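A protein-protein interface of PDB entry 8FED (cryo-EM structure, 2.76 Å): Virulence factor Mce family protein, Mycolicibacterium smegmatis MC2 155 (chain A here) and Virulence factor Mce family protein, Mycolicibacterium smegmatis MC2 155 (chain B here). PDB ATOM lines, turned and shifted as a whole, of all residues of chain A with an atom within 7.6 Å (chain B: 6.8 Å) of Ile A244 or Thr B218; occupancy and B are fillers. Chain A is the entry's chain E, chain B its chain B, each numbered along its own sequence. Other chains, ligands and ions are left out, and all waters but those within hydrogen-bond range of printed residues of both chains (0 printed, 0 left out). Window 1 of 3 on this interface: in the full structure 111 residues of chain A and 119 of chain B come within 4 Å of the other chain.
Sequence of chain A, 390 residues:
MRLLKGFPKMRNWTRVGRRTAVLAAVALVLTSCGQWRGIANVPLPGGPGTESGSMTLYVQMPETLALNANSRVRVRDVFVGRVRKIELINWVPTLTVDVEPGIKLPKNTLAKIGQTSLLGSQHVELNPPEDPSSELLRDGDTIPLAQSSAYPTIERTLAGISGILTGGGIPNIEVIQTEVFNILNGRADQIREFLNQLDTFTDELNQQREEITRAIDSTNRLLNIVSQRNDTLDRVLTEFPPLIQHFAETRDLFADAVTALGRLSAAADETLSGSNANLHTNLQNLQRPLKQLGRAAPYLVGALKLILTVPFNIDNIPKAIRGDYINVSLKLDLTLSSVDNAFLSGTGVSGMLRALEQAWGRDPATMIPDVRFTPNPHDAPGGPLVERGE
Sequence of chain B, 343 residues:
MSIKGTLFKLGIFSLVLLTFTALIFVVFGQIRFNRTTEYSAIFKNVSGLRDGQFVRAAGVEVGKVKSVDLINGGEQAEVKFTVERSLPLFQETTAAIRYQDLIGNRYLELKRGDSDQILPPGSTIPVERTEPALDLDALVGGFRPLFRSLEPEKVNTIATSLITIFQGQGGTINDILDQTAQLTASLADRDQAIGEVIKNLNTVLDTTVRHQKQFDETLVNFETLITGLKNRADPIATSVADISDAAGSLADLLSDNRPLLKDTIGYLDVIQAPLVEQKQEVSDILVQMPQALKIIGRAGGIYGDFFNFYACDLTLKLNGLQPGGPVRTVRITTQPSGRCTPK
O of Glu B217 sits close to OD1 of Asn B221, at 2.8 Å.
Gln B214 touches Pro A241.
CA of Pro A241 touches OG1 of Thr B218 (3.9 Å).
Ile A244 touches Thr B218 (CD1 to OG1, 3.3 Å).
Ile A244 touches Phe B222 (CG2 to N, 3.6 Å).
Glu B217 touches Gln A245 (OE1 to OE1, 3.6 Å).
Asn B221 touches Gln A245 (OD1 to CB, 3.5 Å).
O of Phe A247 touches CD1 of Leu B225, at 3.8 Å.
Asn B221 touches Ala A248.
Of the printed residues of chain B, Pro A241 touches Gln B214 (3.9 Å) and Thr B218 (3.9 Å).
Ile A244 touches two residues of chain B.
Of the printed residues of chain B, Gln A245 touches Glu B217 (3.6 Å) and Asn B221 (3.5 Å).
Of the printed residues of chain B, Phe A247 touches Leu B225.
Of chain A, only Pro A241 (3.9 Å) and Ile A244 (3.3 Å) come within 4 Å of Thr B218.
Of the printed residues of chain A, Phe B222 touches Ile A244 (3.6 Å).
The nearest residue of chain B that does not touch Ile A244 is Asn B221 (4.02 Å).
Printed residues of chain A that touch a printed residue of chain B: Pro A241, Ile A244, Gln A245, Phe A247 and Ala A248.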
ATOM      1  N   LEU A 237     -13.020   7.345 -15.256  1.00  0.00           N
ATOM      2  CA  LEU A 237     -14.055   6.325 -15.144  1.00  0.00           C
ATOM      3  C   LEU A 237     -14.239   5.525 -16.427  1.00  0.00           C
ATOM      4  O   LEU A 237     -14.873   4.465 -16.384  1.00  0.00           O
ATOM      5  CB  LEU A 237     -15.378   6.967 -14.729  1.00  0.00           C
ATOM      6  CG  LEU A 237     -15.401   7.520 -13.302  1.00  0.00           C
ATOM      7  CD1 LEU A 237     -16.712   8.227 -13.011  1.00  0.00           C
ATOM      8  CD2 LEU A 237     -15.166   6.403 -12.301  1.00  0.00           C
ATOM      9  N   GLU A 239     -11.558   4.338 -18.245  1.00  0.00           N
ATOM     10  CA  GLU A 239     -10.404   3.482 -18.506  1.00  0.00           C
ATOM     11  C   GLU A 239      -9.756   2.861 -17.276  1.00  0.00           C
ATOM     12  O   GLU A 239      -9.008   1.888 -17.436  1.00  0.00           O
ATOM     13  CB  GLU A 239      -9.330   4.261 -19.280  1.00  0.00           C
ATOM     14  CG  GLU A 239      -9.793   4.744 -20.647  1.00  0.00           C
ATOM     15  CD  GLU A 239      -8.768   5.615 -21.341  1.00  0.00           C
ATOM     16  OE1 GLU A 239      -7.577   5.532 -20.982  1.00  0.00           O
ATOM     17  OE2 GLU A 239      -9.157   6.389 -22.240  1.00  0.00           O
ATOM     18  N   PHE A 240     -10.000   3.367 -16.068  1.00  0.00           N
ATOM     19  CA  PHE A 240      -9.419   2.769 -14.870  1.00  0.00           C
ATOM     20  C   PHE A 240     -10.145   1.513 -14.377  1.00  0.00           C
ATOM     21  O   PHE A 240      -9.463   0.579 -13.931  1.00  0.00           O
ATOM     22  CB  PHE A 240      -9.346   3.808 -13.746  1.00  0.00           C
ATOM     23  CG  PHE A 240      -7.955   4.277 -13.449  1.00  0.00           C
ATOM     24  CD1 PHE A 240      -6.877   3.424 -13.607  1.00  0.00           C
ATOM     25  CD2 PHE A 240      -7.723   5.571 -13.014  1.00  0.00           C
ATOM     26  CE1 PHE A 240      -5.594   3.851 -13.334  1.00  0.00           C
ATOM     27  CE2 PHE A 240      -6.441   6.003 -12.741  1.00  0.00           C
ATOM     28  CZ  PHE A 240      -5.377   5.142 -12.901  1.00  0.00           C
ATOM     29  N   PRO A 241     -11.483   1.445 -14.375  1.00  0.00           N
ATOM     30  CA  PRO A 241     -12.156   0.216 -13.906  1.00  0.00           C
ATOM     31  C   PRO A 241     -11.715  -1.035 -14.655  1.00  0.00           C
ATOM     32  O   PRO A 241     -11.550  -2.083 -14.013  1.00  0.00           O
ATOM     33  CB  PRO A 241     -13.644   0.520 -14.130  1.00  0.00           C
ATOM     34  CG  PRO A 241     -13.733   1.968 -13.941  1.00  0.00           C
ATOM     35  CD  PRO A 241     -12.467   2.540 -14.519  1.00  0.00           C
ATOM     36  N   PRO A 242     -11.528  -1.008 -15.990  1.00  0.00           N
ATOM     37  CA  PRO A 242     -11.002  -2.228 -16.636  1.00  0.00           C
ATOM     38  C   PRO A 242      -9.618  -2.619 -16.147  1.00  0.00           C
ATOM     39  O   PRO A 242      -9.342  -3.812 -15.962  1.00  0.00           O
ATOM     40  CB  PRO A 242     -10.998  -1.866 -18.127  1.00  0.00           C
ATOM     41  CG  PRO A 242     -12.021  -0.831 -18.262  1.00  0.00           C
ATOM     42  CD  PRO A 242     -11.912  -0.017 -17.017  1.00  0.00           C
ATOM     43  N   LEU A 243      -8.739  -1.638 -15.929  1.00  0.00           N
ATOM     44  CA  LEU A 243      -7.399  -1.933 -15.431  1.00  0.00           C
ATOM     45  C   LEU A 243      -7.459  -2.554 -14.043  1.00  0.00           C
ATOM     46  O   LEU A 243      -6.768  -3.540 -13.759  1.00  0.00           O
ATOM     47  CB  LEU A 243      -6.557  -0.658 -15.409  1.00  0.00           C
ATOM     48  CG  LEU A 243      -5.163  -0.797 -14.797  1.00  0.00           C
ATOM     49  CD1 LEU A 243      -4.246  -1.555 -15.738  1.00  0.00           C
ATOM     50  CD2 LEU A 243      -4.585   0.562 -14.447  1.00  0.00           C
ATOM     51  N   ILE A 244      -8.283  -1.982 -13.161  1.00  0.00           N
ATOM     52  CA  ILE A 244      -8.407  -2.505 -11.803  1.00  0.00           C
ATOM     53  C   ILE A 244      -8.994  -3.910 -11.828  1.00  0.00           C
ATOM     54  O   ILE A 244      -8.551  -4.799 -11.087  1.00  0.00           O
ATOM     55  CB  ILE A 244      -9.244  -1.546 -10.939  1.00  0.00           C
ATOM     56  CG1 ILE A 244      -8.516  -0.210 -10.783  1.00  0.00           C
ATOM     57  CG2 ILE A 244      -9.525  -2.151  -9.579  1.00  0.00           C
ATOM     58  CD1 ILE A 244      -9.231   0.780  -9.896  1.00  0.00           C
ATOM     59  N   GLN A 245      -9.993  -4.138 -12.685  1.00  0.00           N
ATOM     60  CA  GLN A 245     -10.592  -5.462 -12.800  1.00  0.00           C
ATOM     61  C   GLN A 245      -9.575  -6.491 -13.275  1.00  0.00           C
ATOM     62  O   GLN A 245      -9.504  -7.600 -12.731  1.00  0.00           O
ATOM     63  CB  GLN A 245     -11.791  -5.411 -13.747  1.00  0.00           C
ATOM     64  CG  GLN A 245     -12.347  -6.769 -14.123  1.00  0.00           C
ATOM     65  CD  GLN A 245     -13.556  -6.669 -15.030  1.00  0.00           C
ATOM     66  OE1 GLN A 245     -14.313  -5.699 -14.969  1.00  0.00           O
ATOM     67  NE2 GLN A 245     -13.741  -7.670 -15.882  1.00  0.00           N
ATOM     68  N   HIS A 246      -8.768  -6.141 -14.280  1.00  0.00           N
ATOM     69  CA  HIS A 246      -7.774  -7.092 -14.765  1.00  0.00           C
ATOM     70  C   HIS A 246      -6.688  -7.338 -13.727  1.00  0.00           C
ATOM     71  O   HIS A 246      -6.202  -8.466 -13.595  1.00  0.00           O
ATOM     72  CB  HIS A 246      -7.153  -6.616 -16.074  1.00  0.00           C
ATOM     73  CG  HIS A 246      -6.299  -7.652 -16.736  1.00  0.00           C
ATOM     74  ND1 HIS A 246      -6.823  -8.784 -17.320  1.00  0.00           N
ATOM     75  CD2 HIS A 246      -4.957  -7.739 -16.887  1.00  0.00           C
ATOM     76  CE1 HIS A 246      -5.843  -9.519 -17.812  1.00  0.00           C
ATOM     77  NE2 HIS A 246      -4.699  -8.907 -17.563  1.00  0.00           N
ATOM     78  N   PHE A 247      -6.288  -6.298 -12.987  1.00  0.00           N
ATOM     79  CA  PHE A 247      -5.323  -6.494 -11.907  1.00  0.00           C
ATOM     80  C   PHE A 247      -5.873  -7.444 -10.853  1.00  0.00           C
ATOM     81  O   PHE A 247      -5.152  -8.319 -10.358  1.00  0.00           O
ATOM     82  CB  PHE A 247      -4.950  -5.153 -11.275  1.00  0.00           C
ATOM     83  CG  PHE A 247      -3.899  -4.393 -12.032  1.00  0.00           C
ATOM     84  CD1 PHE A 247      -3.206  -4.988 -13.072  1.00  0.00           C
ATOM     85  CD2 PHE A 247      -3.593  -3.086 -11.691  1.00  0.00           C
ATOM     86  CE1 PHE A 247      -2.236  -4.290 -13.765  1.00  0.00           C
ATOM     87  CE2 PHE A 247      -2.624  -2.385 -12.380  1.00  0.00           C
ATOM     88  CZ  PHE A 247      -1.944  -2.987 -13.417  1.00  0.00           C
ATOM     89  N   ALA A 248      -7.148  -7.282 -10.494  1.00  0.00           N
ATOM     90  CA  ALA A 248      -7.786  -8.210  -9.566  1.00  0.00           C
ATOM     91  C   ALA A 248      -7.850  -9.618 -10.139  1.00  0.00           C
ATOM     92  O   ALA A 248      -7.813 -10.597  -9.384  1.00  0.00           O
ATOM     93  CB  ALA A 248      -9.187  -7.719  -9.213  1.00  0.00           C
ATOM     94  N   GLU A 249      -7.959  -9.744 -11.463  1.00  0.00           N
ATOM     95  CA  GLU A 249      -7.945 -11.066 -12.083  1.00  0.00           C
ATOM     96  C   GLU A 249      -6.589 -11.747 -11.932  1.00  0.00           C
ATOM     97  O   GLU A 249      -6.522 -12.970 -11.763  1.00  0.00           O
ATOM     98  CB  GLU A 249      -8.322 -10.959 -13.562  1.00  0.00           C
ATOM     99  CG  GLU A 249      -9.787 -10.644 -13.820  1.00  0.00           C
ATOM    100  CD  GLU A 249     -10.688 -11.852 -13.652  1.00  0.00           C
ATOM    101  OE1 GLU A 249     -10.167 -12.986 -13.618  1.00  0.00           O
ATOM    102  OE2 GLU A 249     -11.919 -11.665 -13.555  1.00  0.00           O
ATOM    103  N   THR A 250      -5.497 -10.981 -11.986  1.00  0.00           N
ATOM    104  CA  THR A 250      -4.153 -11.550 -12.009  1.00  0.00           C
ATOM    105  C   THR A 250      -3.318 -11.110 -10.807  1.00  0.00           C
ATOM    106  O   THR A 250      -2.093 -10.993 -10.903  1.00  0.00           O
ATOM    107  CB  THR A 250      -3.442 -11.198 -13.317  1.00  0.00           C
ATOM    108  OG1 THR A 250      -2.135 -11.781 -13.328  1.00  0.00           O
ATOM    109  CG2 THR A 250      -3.312  -9.690 -13.485  1.00  0.00           C
ATOM    110  N   LYS B 213     -22.285   1.300 -13.519  1.00  0.00           N
ATOM    111  CA  LYS B 213     -21.918  -0.114 -13.516  1.00  0.00           C
ATOM    112  C   LYS B 213     -20.423  -0.292 -13.274  1.00  0.00           C
ATOM    113  O   LYS B 213     -20.006  -1.104 -12.437  1.00  0.00           O
ATOM    114  CB  LYS B 213     -22.333  -0.759 -14.837  1.00  0.00           C
ATOM    115  CG  LYS B 213     -22.277  -2.276 -14.841  1.00  0.00           C
ATOM    116  CD  LYS B 213     -23.353  -2.862 -13.942  1.00  0.00           C
ATOM    117  CE  LYS B 213     -23.519  -4.354 -14.178  1.00  0.00           C
ATOM    118  NZ  LYS B 213     -22.238  -5.093 -14.014  1.00  0.00           N
ATOM    119  N   GLN B 214     -19.599   0.476 -13.991  1.00  0.00           N
ATOM    120  CA  GLN B 214     -18.153   0.358 -13.835  1.00  0.00           C
ATOM    121  C   GLN B 214     -17.703   0.864 -12.472  1.00  0.00           C
ATOM    122  O   GLN B 214     -16.802   0.284 -11.858  1.00  0.00           O
ATOM    123  CB  GLN B 214     -17.442   1.114 -14.957  1.00  0.00           C
ATOM    124  CG  GLN B 214     -18.090   0.955 -16.325  1.00  0.00           C
ATOM    125  CD  GLN B 214     -18.100  -0.481 -16.816  1.00  0.00           C
ATOM    126  OE1 GLN B 214     -17.238  -1.282 -16.453  1.00  0.00           O
ATOM    127  NE2 GLN B 214     -19.079  -0.814 -17.648  1.00  0.00           N
ATOM    128  N   PHE B 215     -18.313   1.948 -11.987  1.00  0.00           N
ATOM    129  CA  PHE B 215     -17.969   2.467 -10.667  1.00  0.00           C
ATOM    130  C   PHE B 215     -18.348   1.483  -9.567  1.00  0.00           C
ATOM    131  O   PHE B 215     -17.686   1.432  -8.527  1.00  0.00           O
ATOM    132  CB  PHE B 215     -18.649   3.817 -10.443  1.00  0.00           C
ATOM    133  CG  PHE B 215     -18.486   4.359  -9.054  1.00  0.00           C
ATOM    134  CD1 PHE B 215     -17.248   4.774  -8.600  1.00  0.00           C
ATOM    135  CD2 PHE B 215     -19.576   4.472  -8.211  1.00  0.00           C
ATOM    136  CE1 PHE B 215     -17.098   5.280  -7.321  1.00  0.00           C
ATOM    137  CE2 PHE B 215     -19.432   4.977  -6.933  1.00  0.00           C
ATOM    138  CZ  PHE B 215     -18.192   5.383  -6.489  1.00  0.00           C
ATOM    139  N   ASP B 216     -19.414   0.708  -9.773  1.00  0.00           N
ATOM    140  CA  ASP B 216     -19.785  -0.312  -8.801  1.00  0.00           C
ATOM    141  C   ASP B 216     -18.836  -1.503  -8.862  1.00  0.00           C
ATOM    142  O   ASP B 216     -18.436  -2.037  -7.821  1.00  0.00           O
ATOM    143  CB  ASP B 216     -21.226  -0.762  -9.041  1.00  0.00           C
ATOM    144  CG  ASP B 216     -21.726  -1.714  -7.976  1.00  0.00           C
ATOM    145  OD1 ASP B 216     -22.069  -1.245  -6.872  1.00  0.00           O
ATOM    146  OD2 ASP B 216     -21.776  -2.933  -8.244  1.00  0.00           O
ATOM    147  N   GLU B 217     -18.467  -1.934 -10.071  1.00  0.00           N
ATOM    148  CA  GLU B 217     -17.589  -3.095 -10.204  1.00  0.00           C
ATOM    149  C   GLU B 217     -16.165  -2.800  -9.746  1.00  0.00           C
ATOM    150  O   GLU B 217     -15.485  -3.699  -9.232  1.00  0.00           O
ATOM    151  CB  GLU B 217     -17.576  -3.586 -11.651  1.00  0.00           C
ATOM    152  CG  GLU B 217     -18.909  -4.110 -12.151  1.00  0.00           C
ATOM    153  CD  GLU B 217     -18.841  -4.585 -13.589  1.00  0.00           C
ATOM    154  OE1 GLU B 217     -17.718  -4.714 -14.121  1.00  0.00           O
ATOM    155  OE2 GLU B 217     -19.909  -4.824 -14.190  1.00  0.00           O
ATOM    156  N   THR B 218     -15.692  -1.562  -9.929  1.00  0.00           N
ATOM    157  CA  THR B 218     -14.301  -1.262  -9.611  1.00  0.00           C
ATOM    158  C   THR B 218     -14.038  -1.305  -8.112  1.00  0.00           C
ATOM    159  O   THR B 218     -12.934  -1.662  -7.701  1.00  0.00           O
ATOM    160  CB  THR B 218     -13.887   0.092 -10.198  1.00  0.00           C
ATOM    161  OG1 THR B 218     -12.487   0.297  -9.975  1.00  0.00           O
ATOM    162  CG2 THR B 218     -14.655   1.236  -9.565  1.00  0.00           C
ATOM    163  N   LEU B 219     -15.028  -0.963  -7.283  1.00  0.00           N
ATOM    164  CA  LEU B 219     -14.847  -1.076  -5.838  1.00  0.00           C
ATOM    165  C   LEU B 219     -14.625  -2.528  -5.430  1.00  0.00           C
ATOM    166  O   LEU B 219     -13.714  -2.834  -4.653  1.00  0.00           O
ATOM    167  CB  LEU B 219     -16.052  -0.486  -5.105  1.00  0.00           C
ATOM    168  CG  LEU B 219     -16.217   1.030  -5.195  1.00  0.00           C
ATOM    169  CD1 LEU B 219     -17.403   1.489  -4.365  1.00  0.00           C
ATOM    170  CD2 LEU B 219     -14.947   1.728  -4.748  1.00  0.00           C
ATOM    171  N   VAL B 220     -15.441  -3.440  -5.966  1.00  0.00           N
ATOM    172  CA  VAL B 220     -15.291  -4.858  -5.655  1.00  0.00           C
ATOM    173  C   VAL B 220     -13.950  -5.378  -6.157  1.00  0.00           C
ATOM    174  O   VAL B 220     -13.244  -6.104  -5.445  1.00  0.00           O
ATOM    175  CB  VAL B 220     -16.461  -5.662  -6.251  1.00  0.00           C
ATOM    176  CG1 VAL B 220     -16.304  -7.141  -5.941  1.00  0.00           C
ATOM    177  CG2 VAL B 220     -17.782  -5.139  -5.726  1.00  0.00           C
ATOM    178  N   ASN B 221     -13.580  -5.019  -7.391  1.00  0.00           N
ATOM    179  CA  ASN B 221     -12.320  -5.506  -7.945  1.00  0.00           C
ATOM    180  C   ASN B 221     -11.125  -4.968  -7.167  1.00  0.00           C
ATOM    181  O   ASN B 221     -10.165  -5.703  -6.900  1.00  0.00           O
ATOM    182  CB  ASN B 221     -12.216  -5.135  -9.424  1.00  0.00           C
ATOM    183  CG  ASN B 221     -13.212  -5.887 -10.281  1.00  0.00           C
ATOM    184  OD1 ASN B 221     -13.997  -5.287 -11.014  1.00  0.00           O
ATOM    185  ND2 ASN B 221     -13.186  -7.211 -10.191  1.00  0.00           N
ATOM    186  N   PHE B 222     -11.164  -3.688  -6.794  1.00  0.00           N
ATOM    187  CA  PHE B 222     -10.077  -3.101  -6.023  1.00  0.00           C
ATOM    188  C   PHE B 222      -9.980  -3.737  -4.645  1.00  0.00           C
ATOM    189  O   PHE B 222      -8.876  -3.988  -4.153  1.00  0.00           O
ATOM    190  CB  PHE B 222     -10.275  -1.591  -5.912  1.00  0.00           C
ATOM    191  CG  PHE B 222      -8.992  -0.816  -5.807  1.00  0.00           C
ATOM    192  CD1 PHE B 222      -7.769  -1.462  -5.843  1.00  0.00           C
ATOM    193  CD2 PHE B 222      -9.013   0.561  -5.671  1.00  0.00           C
ATOM    194  CE1 PHE B 222      -6.592  -0.751  -5.748  1.00  0.00           C
ATOM    195  CE2 PHE B 222      -7.838   1.278  -5.574  1.00  0.00           C
ATOM    196  CZ  PHE B 222      -6.626   0.622  -5.612  1.00  0.00           C
ATOM    197  N   GLU B 223     -11.123  -4.001  -4.002  1.00  0.00           N
ATOM    198  CA  GLU B 223     -11.100  -4.679  -2.712  1.00  0.00           C
ATOM    199  C   GLU B 223     -10.495  -6.069  -2.838  1.00  0.00           C
ATOM    200  O   GLU B 223      -9.694  -6.482  -1.992  1.00  0.00           O
ATOM    201  CB  GLU B 223     -12.514  -4.750  -2.130  1.00  0.00           C
ATOM    202  CG  GLU B 223     -12.624  -5.441  -0.773  1.00  0.00           C
ATOM    203  CD  GLU B 223     -12.837  -6.941  -0.877  1.00  0.00           C
ATOM    204  OE1 GLU B 223     -13.135  -7.428  -1.987  1.00  0.00           O
ATOM    205  OE2 GLU B 223     -12.702  -7.635   0.153  1.00  0.00           O
ATOM    206  N   THR B 224     -10.866  -6.804  -3.889  1.00  0.00           N
ATOM    207  CA  THR B 224     -10.305  -8.137  -4.092  1.00  0.00           C
ATOM    208  C   THR B 224      -8.796  -8.073  -4.301  1.00  0.00           C
ATOM    209  O   THR B 224      -8.046  -8.862  -3.714  1.00  0.00           O
ATOM    210  CB  THR B 224     -10.984  -8.814  -5.283  1.00  0.00           C
ATOM    211  OG1 THR B 224     -12.395  -8.885  -5.050  1.00  0.00           O
ATOM    212  CG2 THR B 224     -10.442 -10.219  -5.477  1.00  0.00           C
ATOM    213  N   LEU B 225      -8.334  -7.125  -5.123  1.00  0.00           N
ATOM    214  CA  LEU B 225      -6.902  -6.985  -5.373  1.00  0.00           C
ATOM    215  C   LEU B 225      -6.146  -6.617  -4.102  1.00  0.00           C
ATOM    216  O   LEU B 225      -5.088  -7.188  -3.808  1.00  0.00           O
ATOM    217  CB  LEU B 225      -6.666  -5.935  -6.459  1.00  0.00           C
ATOM    218  CG  LEU B 225      -5.238  -5.418  -6.633  1.00  0.00           C
ATOM    219  CD1 LEU B 225      -4.314  -6.521  -7.114  1.00  0.00           C
ATOM    220  CD2 LEU B 225      -5.214  -4.237  -7.588  1.00  0.00           C
